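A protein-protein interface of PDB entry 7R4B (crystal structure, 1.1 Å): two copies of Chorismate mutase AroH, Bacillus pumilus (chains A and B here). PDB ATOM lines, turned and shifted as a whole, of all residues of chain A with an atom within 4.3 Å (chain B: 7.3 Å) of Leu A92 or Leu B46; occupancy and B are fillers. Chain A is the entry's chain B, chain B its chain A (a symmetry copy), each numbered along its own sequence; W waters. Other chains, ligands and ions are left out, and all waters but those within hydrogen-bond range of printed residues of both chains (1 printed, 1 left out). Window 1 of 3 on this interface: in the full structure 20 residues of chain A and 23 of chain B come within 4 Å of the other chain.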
ATOM      1  N   GLY A   5      11.326 -14.383  14.500  1.00  0.00           N
ATOM      2  CA  GLY A   5      11.465 -14.464  15.941  1.00  0.00           C
ATOM      3  C   GLY A   5      10.929 -15.772  16.491  1.00  0.00           C
ATOM      4  O   GLY A   5       9.910 -16.283  16.032  1.00  0.00           O
ATOM      5  N   ILE A   6      11.638 -16.312  17.487  1.00  0.00           N
ATOM      6  CA  ILE A   6      11.228 -17.515  18.199  1.00  0.00           C
ATOM      7  C   ILE A   6      11.086 -17.142  19.659  1.00  0.00           C
ATOM      8  O   ILE A   6      12.046 -16.653  20.274  1.00  0.00           O
ATOM      9  CB  ILE A   6      12.203 -18.684  18.032  1.00  0.00           C
ATOM     10  CG1 ILE A   6      12.619 -18.875  16.573  1.00  0.00           C
ATOM     11  CG2 ILE A   6      11.550 -19.956  18.604  1.00  0.00           C
ATOM     12  CD1 ILE A   6      13.605 -20.031  16.386  1.00  0.00           C
ATOM     13  N   ARG A   7       9.902 -17.391  20.211  1.00  0.00           N
ATOM     14  CA  ARG A   7       9.618 -17.095  21.606  1.00  0.00           C
ATOM     15  C   ARG A   7       9.756 -18.318  22.492  1.00  0.00           C
ATOM     16  O   ARG A   7       9.430 -19.444  22.108  1.00  0.00           O
ATOM     17  CB  ARG A   7       8.185 -16.572  21.745  1.00  0.00           C
ATOM     18  CG  ARG A   7       7.951 -15.126  21.329  1.00  0.00           C
ATOM     19  CD  ARG A   7       8.430 -14.078  22.356  1.00  0.00           C
ATOM     20  NE  ARG A   7       8.492 -14.563  23.731  1.00  0.00           N
ATOM     21  CZ  ARG A   7       7.467 -14.577  24.574  1.00  0.00           C
ATOM     22  NH1 ARG A   7       6.296 -14.059  24.244  1.00  0.00           N
ATOM     23  NH2 ARG A   7       7.620 -15.147  25.767  1.00  0.00           N
ATOM     24  N   GLN A  44      20.457 -12.271  17.054  1.00  0.00           N
ATOM     25  CA  GLN A  44      20.502 -11.757  18.411  1.00  0.00           C
ATOM     26  C   GLN A  44      19.445 -12.479  19.230  1.00  0.00           C
ATOM     27  O   GLN A  44      18.509 -13.078  18.689  1.00  0.00           O
ATOM     28  CB  GLN A  44      20.252 -10.249  18.451  1.00  0.00           C
ATOM     29  CG  GLN A  44      18.872  -9.898  17.961  1.00  0.00           C
ATOM     30  CD  GLN A  44      18.679  -8.448  17.736  1.00  0.00           C
ATOM     31  OE1 GLN A  44      19.515  -7.787  17.105  1.00  0.00           O
ATOM     32  NE2 GLN A  44      17.574  -7.909  18.284  1.00  0.00           N
ATOM     33  N   ILE A  45      19.601 -12.385  20.549  1.00  0.00           N
ATOM     34  CA  ILE A  45      18.647 -12.905  21.514  1.00  0.00           C
ATOM     35  C   ILE A  45      18.342 -11.800  22.512  1.00  0.00           C
ATOM     36  O   ILE A  45      19.261 -11.167  23.044  1.00  0.00           O
ATOM     37  CB  ILE A  45      19.206 -14.112  22.292  1.00  0.00           C
ATOM     38  CG1 ILE A  45      19.807 -15.167  21.369  1.00  0.00           C
ATOM     39  CG2 ILE A  45      18.125 -14.711  23.172  1.00  0.00           C
ATOM     40  CD1 ILE A  45      20.492 -16.305  22.121  1.00  0.00           C
ATOM     41  N   LEU A  46      17.063 -11.636  22.831  1.00  0.00           N
ATOM     42  CA  LEU A  46      16.628 -10.842  23.972  1.00  0.00           C
ATOM     43  C   LEU A  46      16.053 -11.775  25.032  1.00  0.00           C
ATOM     44  O   LEU A  46      15.333 -12.727  24.709  1.00  0.00           O
ATOM     45  CB  LEU A  46      15.536  -9.843  23.591  1.00  0.00           C
ATOM     46  CG  LEU A  46      15.925  -8.807  22.548  1.00  0.00           C
ATOM     47  CD1 LEU A  46      14.710  -8.002  22.118  1.00  0.00           C
ATOM     48  CD2 LEU A  46      17.008  -7.904  23.126  1.00  0.00           C
ATOM     49  N   VAL A  91      12.199 -15.490  26.356  1.00  0.00           N
ATOM     50  CA  VAL A  91      13.212 -15.380  25.313  1.00  0.00           C
ATOM     51  C   VAL A  91      12.562 -14.939  24.012  1.00  0.00           C
ATOM     52  O   VAL A  91      11.466 -15.391  23.677  1.00  0.00           O
ATOM     53  CB  VAL A  91      13.881 -16.761  25.122  1.00  0.00           C
ATOM     54  CG1 VAL A  91      14.736 -16.801  23.869  1.00  0.00           C
ATOM     55  CG2 VAL A  91      14.667 -17.158  26.395  1.00  0.00           C
ATOM     56  N   LEU A  92      13.269 -14.093  23.258  1.00  0.00           N
ATOM     57  CA  LEU A  92      12.923 -13.776  21.876  1.00  0.00           C
ATOM     58  C   LEU A  92      14.216 -13.848  21.068  1.00  0.00           C
ATOM     59  O   LEU A  92      15.091 -12.985  21.173  1.00  0.00           O
ATOM     60  CB  LEU A  92      12.262 -12.411  21.766  1.00  0.00           C
ATOM     61  CG  LEU A  92      11.889 -11.941  20.361  1.00  0.00           C
ATOM     62  CD1 LEU A  92      10.954 -12.908  19.680  1.00  0.00           C
ATOM     63  CD2 LEU A  92      11.255 -10.562  20.467  1.00  0.00           C
ATOM     64  N   MET A  93      14.369 -14.932  20.329  1.00  0.00           N
ATOM     65  CA  MET A  93      15.540 -15.220  19.518  1.00  0.00           C
ATOM     66  C   MET A  93      15.219 -14.938  18.054  1.00  0.00           C
ATOM     67  O   MET A  93      14.235 -15.455  17.536  1.00  0.00           O
ATOM     68  CB  MET A  93      15.876 -16.707  19.697  1.00  0.00           C
ATOM     69  CG  MET A  93      17.155 -17.161  19.058  1.00  0.00           C
ATOM     70  SD  MET A  93      17.406 -18.952  19.128  1.00  0.00           S
ATOM     71  CE  MET A  93      17.714 -19.169  20.914  1.00  0.00           C
ATOM     72  N   THR A  94      16.074 -14.171  17.379  1.00  0.00           N
ATOM     73  CA  THR A  94      15.852 -13.805  15.982  1.00  0.00           C
ATOM     74  C   THR A  94      16.792 -14.635  15.110  1.00  0.00           C
ATOM     75  O   THR A  94      18.012 -14.563  15.276  1.00  0.00           O
ATOM     76  CB  THR A  94      16.114 -12.314  15.777  1.00  0.00           C
ATOM     77  OG1 THR A  94      15.359 -11.536  16.709  1.00  0.00           O
ATOM     78  CG2 THR A  94      15.739 -11.920  14.336  1.00  0.00           C
ATOM     79  N   ILE B   6      10.023  -0.393  12.739  1.00  0.00           N
ATOM     80  CA  ILE B   6       8.968   0.613  12.647  1.00  0.00           C
ATOM     81  C   ILE B   6       8.567   0.962  14.078  1.00  0.00           C
ATOM     82  O   ILE B   6       8.202   0.071  14.861  1.00  0.00           O
ATOM     83  CB  ILE B   6       7.749   0.120  11.856  1.00  0.00           C
ATOM     84  CG1 ILE B   6       8.160  -0.502  10.530  1.00  0.00           C
ATOM     85  CG2 ILE B   6       6.791   1.308  11.695  1.00  0.00           C
ATOM     86  CD1 ILE B   6       6.968  -0.937   9.669  1.00  0.00           C
ATOM     87  N   GLY B   8       6.313   3.062  17.012  1.00  0.00           N
ATOM     88  CA  GLY B   8       5.104   3.783  17.349  1.00  0.00           C
ATOM     89  C   GLY B   8       5.127   4.174  18.811  1.00  0.00           C
ATOM     90  O   GLY B   8       5.804   3.548  19.625  1.00  0.00           O
ATOM     91  N   LEU B  28      -1.217   0.059  16.809  1.00  0.00           N
ATOM     92  CA  LEU B  28      -0.845  -1.006  15.885  1.00  0.00           C
ATOM     93  C   LEU B  28      -1.594  -0.868  14.567  1.00  0.00           C
ATOM     94  O   LEU B  28      -1.004  -1.023  13.498  1.00  0.00           O
ATOM     95  CB  LEU B  28      -1.111  -2.372  16.524  1.00  0.00           C
ATOM     96  CG  LEU B  28      -0.178  -2.752  17.663  1.00  0.00           C
ATOM     97  CD1 LEU B  28      -0.724  -3.967  18.400  1.00  0.00           C
ATOM     98  CD2 LEU B  28       1.210  -3.021  17.146  1.00  0.00           C
ATOM     99  N   VAL B  43       8.804 -10.074  11.500  1.00  0.00           N
ATOM    100  CA  VAL B  43       9.742 -10.940  12.213  1.00  0.00           C
ATOM    101  C   VAL B  43       9.332 -11.077  13.669  1.00  0.00           C
ATOM    102  O   VAL B  43       9.284 -12.187  14.214  1.00  0.00           O
ATOM    103  CB  VAL B  43      11.159 -10.360  12.091  1.00  0.00           C
ATOM    104  CG1 VAL B  43      12.144 -11.200  12.885  1.00  0.00           C
ATOM    105  CG2 VAL B  43      11.574 -10.253  10.635  1.00  0.00           C
ATOM    106  N   GLN B  44       9.045  -9.946  14.320  1.00  0.00           N
ATOM    107  CA  GLN B  44       8.749  -9.874  15.745  1.00  0.00           C
ATOM    108  C   GLN B  44       8.310  -8.458  16.079  1.00  0.00           C
ATOM    109  O   GLN B  44       8.548  -7.515  15.321  1.00  0.00           O
ATOM    110  CB  GLN B  44       9.969 -10.262  16.573  1.00  0.00           C
ATOM    111  CG  GLN B  44      11.134  -9.335  16.407  1.00  0.00           C
ATOM    112  CD  GLN B  44      12.408  -9.945  16.898  1.00  0.00           C
ATOM    113  OE1 GLN B  44      12.741 -11.101  16.590  1.00  0.00           O
ATOM    114  NE2 GLN B  44      13.073  -9.219  17.755  1.00  0.00           N
ATOM    115  N   ILE B  45       7.678  -8.330  17.235  1.00  0.00           N
ATOM    116  CA  ILE B  45       7.279  -7.034  17.771  1.00  0.00           C
ATOM    117  C   ILE B  45       7.758  -6.940  19.210  1.00  0.00           C
ATOM    118  O   ILE B  45       7.569  -7.878  19.994  1.00  0.00           O
ATOM    119  CB  ILE B  45       5.743  -6.876  17.778  1.00  0.00           C
ATOM    120  CG1 ILE B  45       5.129  -7.219  16.419  1.00  0.00           C
ATOM    121  CG2 ILE B  45       5.339  -5.486  18.212  1.00  0.00           C
ATOM    122  CD1 ILE B  45       3.603  -7.231  16.464  1.00  0.00           C
ATOM    123  N   LEU B  46       8.292  -5.778  19.579  1.00  0.00           N
ATOM    124  CA  LEU B  46       8.544  -5.425  20.972  1.00  0.00           C
ATOM    125  C   LEU B  46       7.616  -4.292  21.380  1.00  0.00           C
ATOM    126  O   LEU B  46       7.366  -3.391  20.579  1.00  0.00           O
ATOM    127  CB  LEU B  46       9.965  -4.903  21.158  1.00  0.00           C
ATOM    128  CG  LEU B  46      11.074  -5.894  20.902  1.00  0.00           C
ATOM    129  CD1 LEU B  46      12.439  -5.204  20.955  1.00  0.00           C
ATOM    130  CD2 LEU B  46      11.035  -7.026  21.936  1.00  0.00           C
ATOM    131  N   ILE B  47       7.085  -4.366  22.598  1.00  0.00           N
ATOM    132  CA  ILE B  47       6.237  -3.287  23.114  1.00  0.00           C
ATOM    133  C   ILE B  47       6.745  -2.934  24.507  1.00  0.00           C
ATOM    134  O   ILE B  47       6.793  -3.803  25.383  1.00  0.00           O
ATOM    135  CB  ILE B  47       4.743  -3.660  23.173  1.00  0.00           C
ATOM    136  CG1 ILE B  47       4.266  -4.244  21.849  1.00  0.00           C
ATOM    137  CG2 ILE B  47       3.945  -2.429  23.597  1.00  0.00           C
ATOM    138  CD1 ILE B  47       2.808  -4.693  21.828  1.00  0.00           C
ATOM    139  N   SER B  48       7.109  -1.672  24.721  1.00  0.00           N
ATOM    140  CA  SER B  48       7.454  -1.206  26.057  1.00  0.00           C
ATOM    141  C   SER B  48       6.307  -0.414  26.661  1.00  0.00           C
ATOM    142  O   SER B  48       5.458   0.145  25.961  1.00  0.00           O
ATOM    143  CB  SER B  48       8.718  -0.353  26.068  1.00  0.00           C
ATOM    144  OG  SER B  48       8.467   0.938  25.555  1.00  0.00           O
ATOM    145  N   PRO B  72       5.386 -13.185  16.657  1.00  0.00           N
ATOM    146  CA  PRO B  72       5.907 -13.169  18.029  1.00  0.00           C
ATOM    147  C   PRO B  72       5.977 -11.757  18.574  1.00  0.00           C
ATOM    148  O   PRO B  72       6.380 -10.818  17.884  1.00  0.00           O
ATOM    149  CB  PRO B  72       7.292 -13.811  17.911  1.00  0.00           C
ATOM    150  CG  PRO B  72       7.641 -13.783  16.490  1.00  0.00           C
ATOM    151  CD  PRO B  72       6.417 -13.525  15.662  1.00  0.00           C
ATOM    152  N   VAL B  73       5.567 -11.622  19.828  1.00  0.00           N
ATOM    153  CA  VAL B  73       5.539 -10.329  20.498  1.00  0.00           C
ATOM    154  C   VAL B  73       5.952 -10.527  21.943  1.00  0.00           C
ATOM    155  O   VAL B  73       5.604 -11.531  22.577  1.00  0.00           O
ATOM    156  CB  VAL B  73       4.151  -9.655  20.374  1.00  0.00           C
ATOM    157  CG1 VAL B  73       3.056 -10.551  20.918  1.00  0.00           C
ATOM    158  CG2 VAL B  73       4.122  -8.288  21.078  1.00  0.00           C
ATOM    159  N   THR B  74       6.689  -9.559  22.476  1.00  0.00           N
ATOM    160  CA  THR B  74       6.970  -9.597  23.906  1.00  0.00           C
ATOM    161  C   THR B  74       7.172  -8.162  24.375  1.00  0.00           C
ATOM    162  O   THR B  74       7.417  -7.252  23.563  1.00  0.00           O
ATOM    163  CB  THR B  74       8.142 -10.548  24.186  1.00  0.00           C
ATOM    164  OG1 THR B  74       8.075 -11.033  25.536  1.00  0.00           O
ATOM    165  CG2 THR B  74       9.467  -9.846  23.984  1.00  0.00           C
ATOM    166  N   CYS B  75       7.118  -7.978  25.691  1.00  0.00           N
ATOM    167  CA  CYS B  75       7.120  -6.656  26.294  1.00  0.00           C
ATOM    168  C   CYS B  75       8.362  -6.406  27.144  1.00  0.00           C
ATOM    169  O   CYS B  75       9.148  -7.299  27.457  1.00  0.00           O
ATOM    170  CB  CYS B  75       5.847  -6.421  27.125  1.00  0.00           C
ATOM    171  SG  CYS B  75       4.310  -6.620  26.172  1.00  0.00           S
ATOM    172  N   MET B  76       8.511  -5.140  27.524  1.00  0.00           N
ATOM    173  CA  MET B  76       9.634  -4.717  28.345  1.00  0.00           C
ATOM    174  C   MET B  76       9.280  -3.412  29.039  1.00  0.00           C
ATOM    175  O   MET B  76       8.546  -2.594  28.490  1.00  0.00           O
ATOM    176  CB  MET B  76      10.902  -4.551  27.496  1.00  0.00           C
ATOM    177  CG  MET B  76      10.784  -3.501  26.403  1.00  0.00           C
ATOM    178  SD  MET B  76      12.015  -3.714  25.116  1.00  0.00           S
ATOM    179  CE  MET B  76      11.791  -2.207  24.181  1.00  0.00           C
ATOM    180  N   ARG B  90       5.138   2.110  23.802  1.00  0.00           N
ATOM    181  CA  ARG B  90       5.968   2.266  22.609  1.00  0.00           C
ATOM    182  C   ARG B  90       6.144   0.927  21.910  1.00  0.00           C
ATOM    183  O   ARG B  90       6.369  -0.095  22.554  1.00  0.00           O
ATOM    184  CB  ARG B  90       7.352   2.826  22.977  1.00  0.00           C
ATOM    185  CG  ARG B  90       7.324   4.252  23.497  1.00  0.00           C
ATOM    186  CD  ARG B  90       8.653   4.669  24.104  1.00  0.00           C
ATOM    187  NE  ARG B  90       8.751   6.080  24.476  1.00  0.00           N
ATOM    188  CZ  ARG B  90       8.532   6.572  25.685  1.00  0.00           C
ATOM    189  NH1 ARG B  90       8.026   5.842  26.654  1.00  0.00           N
ATOM    190  NH2 ARG B  90       8.826   7.843  25.929  1.00  0.00           N
ATOM    191  N   VAL B  91       6.055   0.937  20.593  1.00  0.00           N
ATOM    192  CA  VAL B  91       6.164  -0.263  19.770  1.00  0.00           C
ATOM    193  C   VAL B  91       7.415  -0.174  18.910  1.00  0.00           C
ATOM    194  O   VAL B  91       7.757   0.897  18.393  1.00  0.00           O
ATOM    195  CB  VAL B  91       4.918  -0.368  18.868  1.00  0.00           C
ATOM    196  CG1 VAL B  91       5.079  -1.474  17.821  1.00  0.00           C
ATOM    197  CG2 VAL B  91       3.664  -0.589  19.686  1.00  0.00           C
ATOM    198  N   LEU B  92       8.089  -1.308  18.741  1.00  0.00           N
ATOM    199  CA  LEU B  92       9.170  -1.469  17.764  1.00  0.00           C
ATOM    200  C   LEU B  92       8.870  -2.772  17.021  1.00  0.00           C
ATOM    201  O   LEU B  92       9.056  -3.865  17.559  1.00  0.00           O
ATOM    202  CB  LEU B  92      10.539  -1.484  18.429  1.00  0.00           C
ATOM    203  CG  LEU B  92      11.718  -1.639  17.466  1.00  0.00           C
ATOM    204  CD1 LEU B  92      11.811  -0.559  16.420  1.00  0.00           C
ATOM    205  CD2 LEU B  92      13.007  -1.712  18.285  1.00  0.00           C
ATOM    206  N   MET B  93       8.346  -2.648  15.807  1.00  0.00           N
ATOM    207  CA  MET B  93       7.941  -3.776  14.981  1.00  0.00           C
ATOM    208  C   MET B  93       8.991  -3.968  13.893  1.00  0.00           C
ATOM    209  O   MET B  93       9.314  -3.021  13.177  1.00  0.00           O
ATOM    210  CB  MET B  93       6.570  -3.480  14.352  1.00  0.00           C
ATOM    211  CG  MET B  93       6.055  -4.528  13.412  1.00  0.00           C
ATOM    212  SD  MET B  93       4.469  -4.108  12.673  1.00  0.00           S
ATOM    213  CE  MET B  93       3.321  -3.866  14.034  1.00  0.00           C
ATOM    214  N   THR B  94       9.488  -5.198  13.741  1.00  0.00           N
ATOM    215  CA  THR B  94      10.534  -5.499  12.765  1.00  0.00           C
ATOM    216  C   THR B  94       9.881  -6.180  11.578  1.00  0.00           C
ATOM    217  O   THR B  94       9.343  -7.278  11.718  1.00  0.00           O
ATOM    218  CB  THR B  94      11.618  -6.396  13.359  1.00  0.00           C
ATOM    219  OG1 THR B  94      12.155  -5.783  14.539  1.00  0.00           O
ATOM    220  CG2 THR B  94      12.733  -6.602  12.374  1.00  0.00           C
HETATM  221  O   HOH W   1      15.630 -10.791  19.322  1.00  0.00           O
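The backbone NH of Gly A5 sits at hydrogen-bond distance from the backbone carbonyl oxygen of Val B43, at 3.0 Å.
The guanidinium group (NH1) of Arg A7 is in hydrogen-bond range of the backbone carbonyl oxygen (O) of Val B73, at 3.1 Å.
OG1 of Thr A94 lies within hydrogen-bond range of OE1 of Gln B44 (2.7 Å).
O of Gln A44 is in hydrogen-bond range of N of Thr A94 (3.0 Å).
The backbone NH (N) of Val B43 sits at hydrogen-bond distance from the backbone carbonyl oxygen (O) of Thr B94, 2.9 Å away.
The backbone carbonyl oxygen (O) of Gln B44 is in hydrogen-bond range of the backbone NH (N) of Thr B94.
N of Ile B45 is in hydrogen-bond range of O of Pro B72, at 2.9 Å.
The backbone NH of Leu B92 lies within hydrogen-bond range of the backbone carbonyl oxygen of Leu B46.
N of Ile B47 is in hydrogen-bond range of O of Thr B74, at 3.1 Å.
OE1 of Gln B44 touches CA of Gly A5, 3.7 Å away.
O of Gly A5 touches CG of Pro B72, at 3.4 Å.
Arg A7 touches Pro B72 (CG to CB, 3.7 Å).
Arg A7 touches Thr B74.
Leu A46 touches Leu B46.
Leu A92 touches Gln B44 (CD2 to NE2, 3.5 Å).
Leu A92 touches Leu B46 (CD2 to CD2, 3.8 Å).
Val B43 touches Thr A94 (CG1 to CG2, 3.9 Å).
Printed residues of chain B within 4 Å of Leu A92: Gln B44 and Leu B46.
Of chain A, only Leu A46 and Leu A92 come within 4 Å of Leu B46.
Of the printed residues of chain A, Thr B74 touches Arg A7 (3.7 Å).
Of the printed residues of chain A, Val B73 touches Arg A7 (3.1 Å).
Of the printed residues of chain A, Gln B44 touches Gly A5 (3.7 Å), Leu A92 (3.5 Å) and Thr A94 (2.7 Å).
Printed residues of chain B within 4 Å of Arg A7: Pro B72, Val B73 and Thr B74.
Of the printed residues of chain A, Pro B72 touches Gly A5 (3.4 Å) and Arg A7 (3.7 Å).
Met B76 touches none of the printed residues of chain A.
Met B93 touches none of the printed residues of chain A.
Printed residues of chain A that touch a printed residue of chain B: Gly A5, Arg A7, Leu A46, Leu A92 and Thr A94.
Along chain A the printed residues that touch a printed residue of chain B span positions 5 to 94.
Hydrophobic or aromatic side chains of chain B within 4 Å of the printed part of chain A: Val B43, Leu B46 and Pro B72.
Among the printed residues, 11 pairs touch across the chains.
Among the printed residues, no Asp or Glu carboxylate lies within 4 Å of a Lys or Arg side-chain nitrogen of the other chain.
Leu B46 touches its own counterpart, Leu A46.
Leu A92 touches Gln B44, but with the chains exchanged Gln A44 does not touch Leu B92 (7.7 Å).
Leu A92 touches Leu B46, but with the chains exchanged Leu A46 does not touch Leu B92 (7.6 Å).
Thr A94 touches Gln B44, but with the chains exchanged Gln A44 does not touch Thr B94 (6.9 Å).
8 positions are printed for both chains.
Water W1 lies within hydrogen-bond range of OG1 of Thr A94 (2.7 Å), O of Leu A92 (2.9 Å) and NE2 of Gln B44 (3.4 Å).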
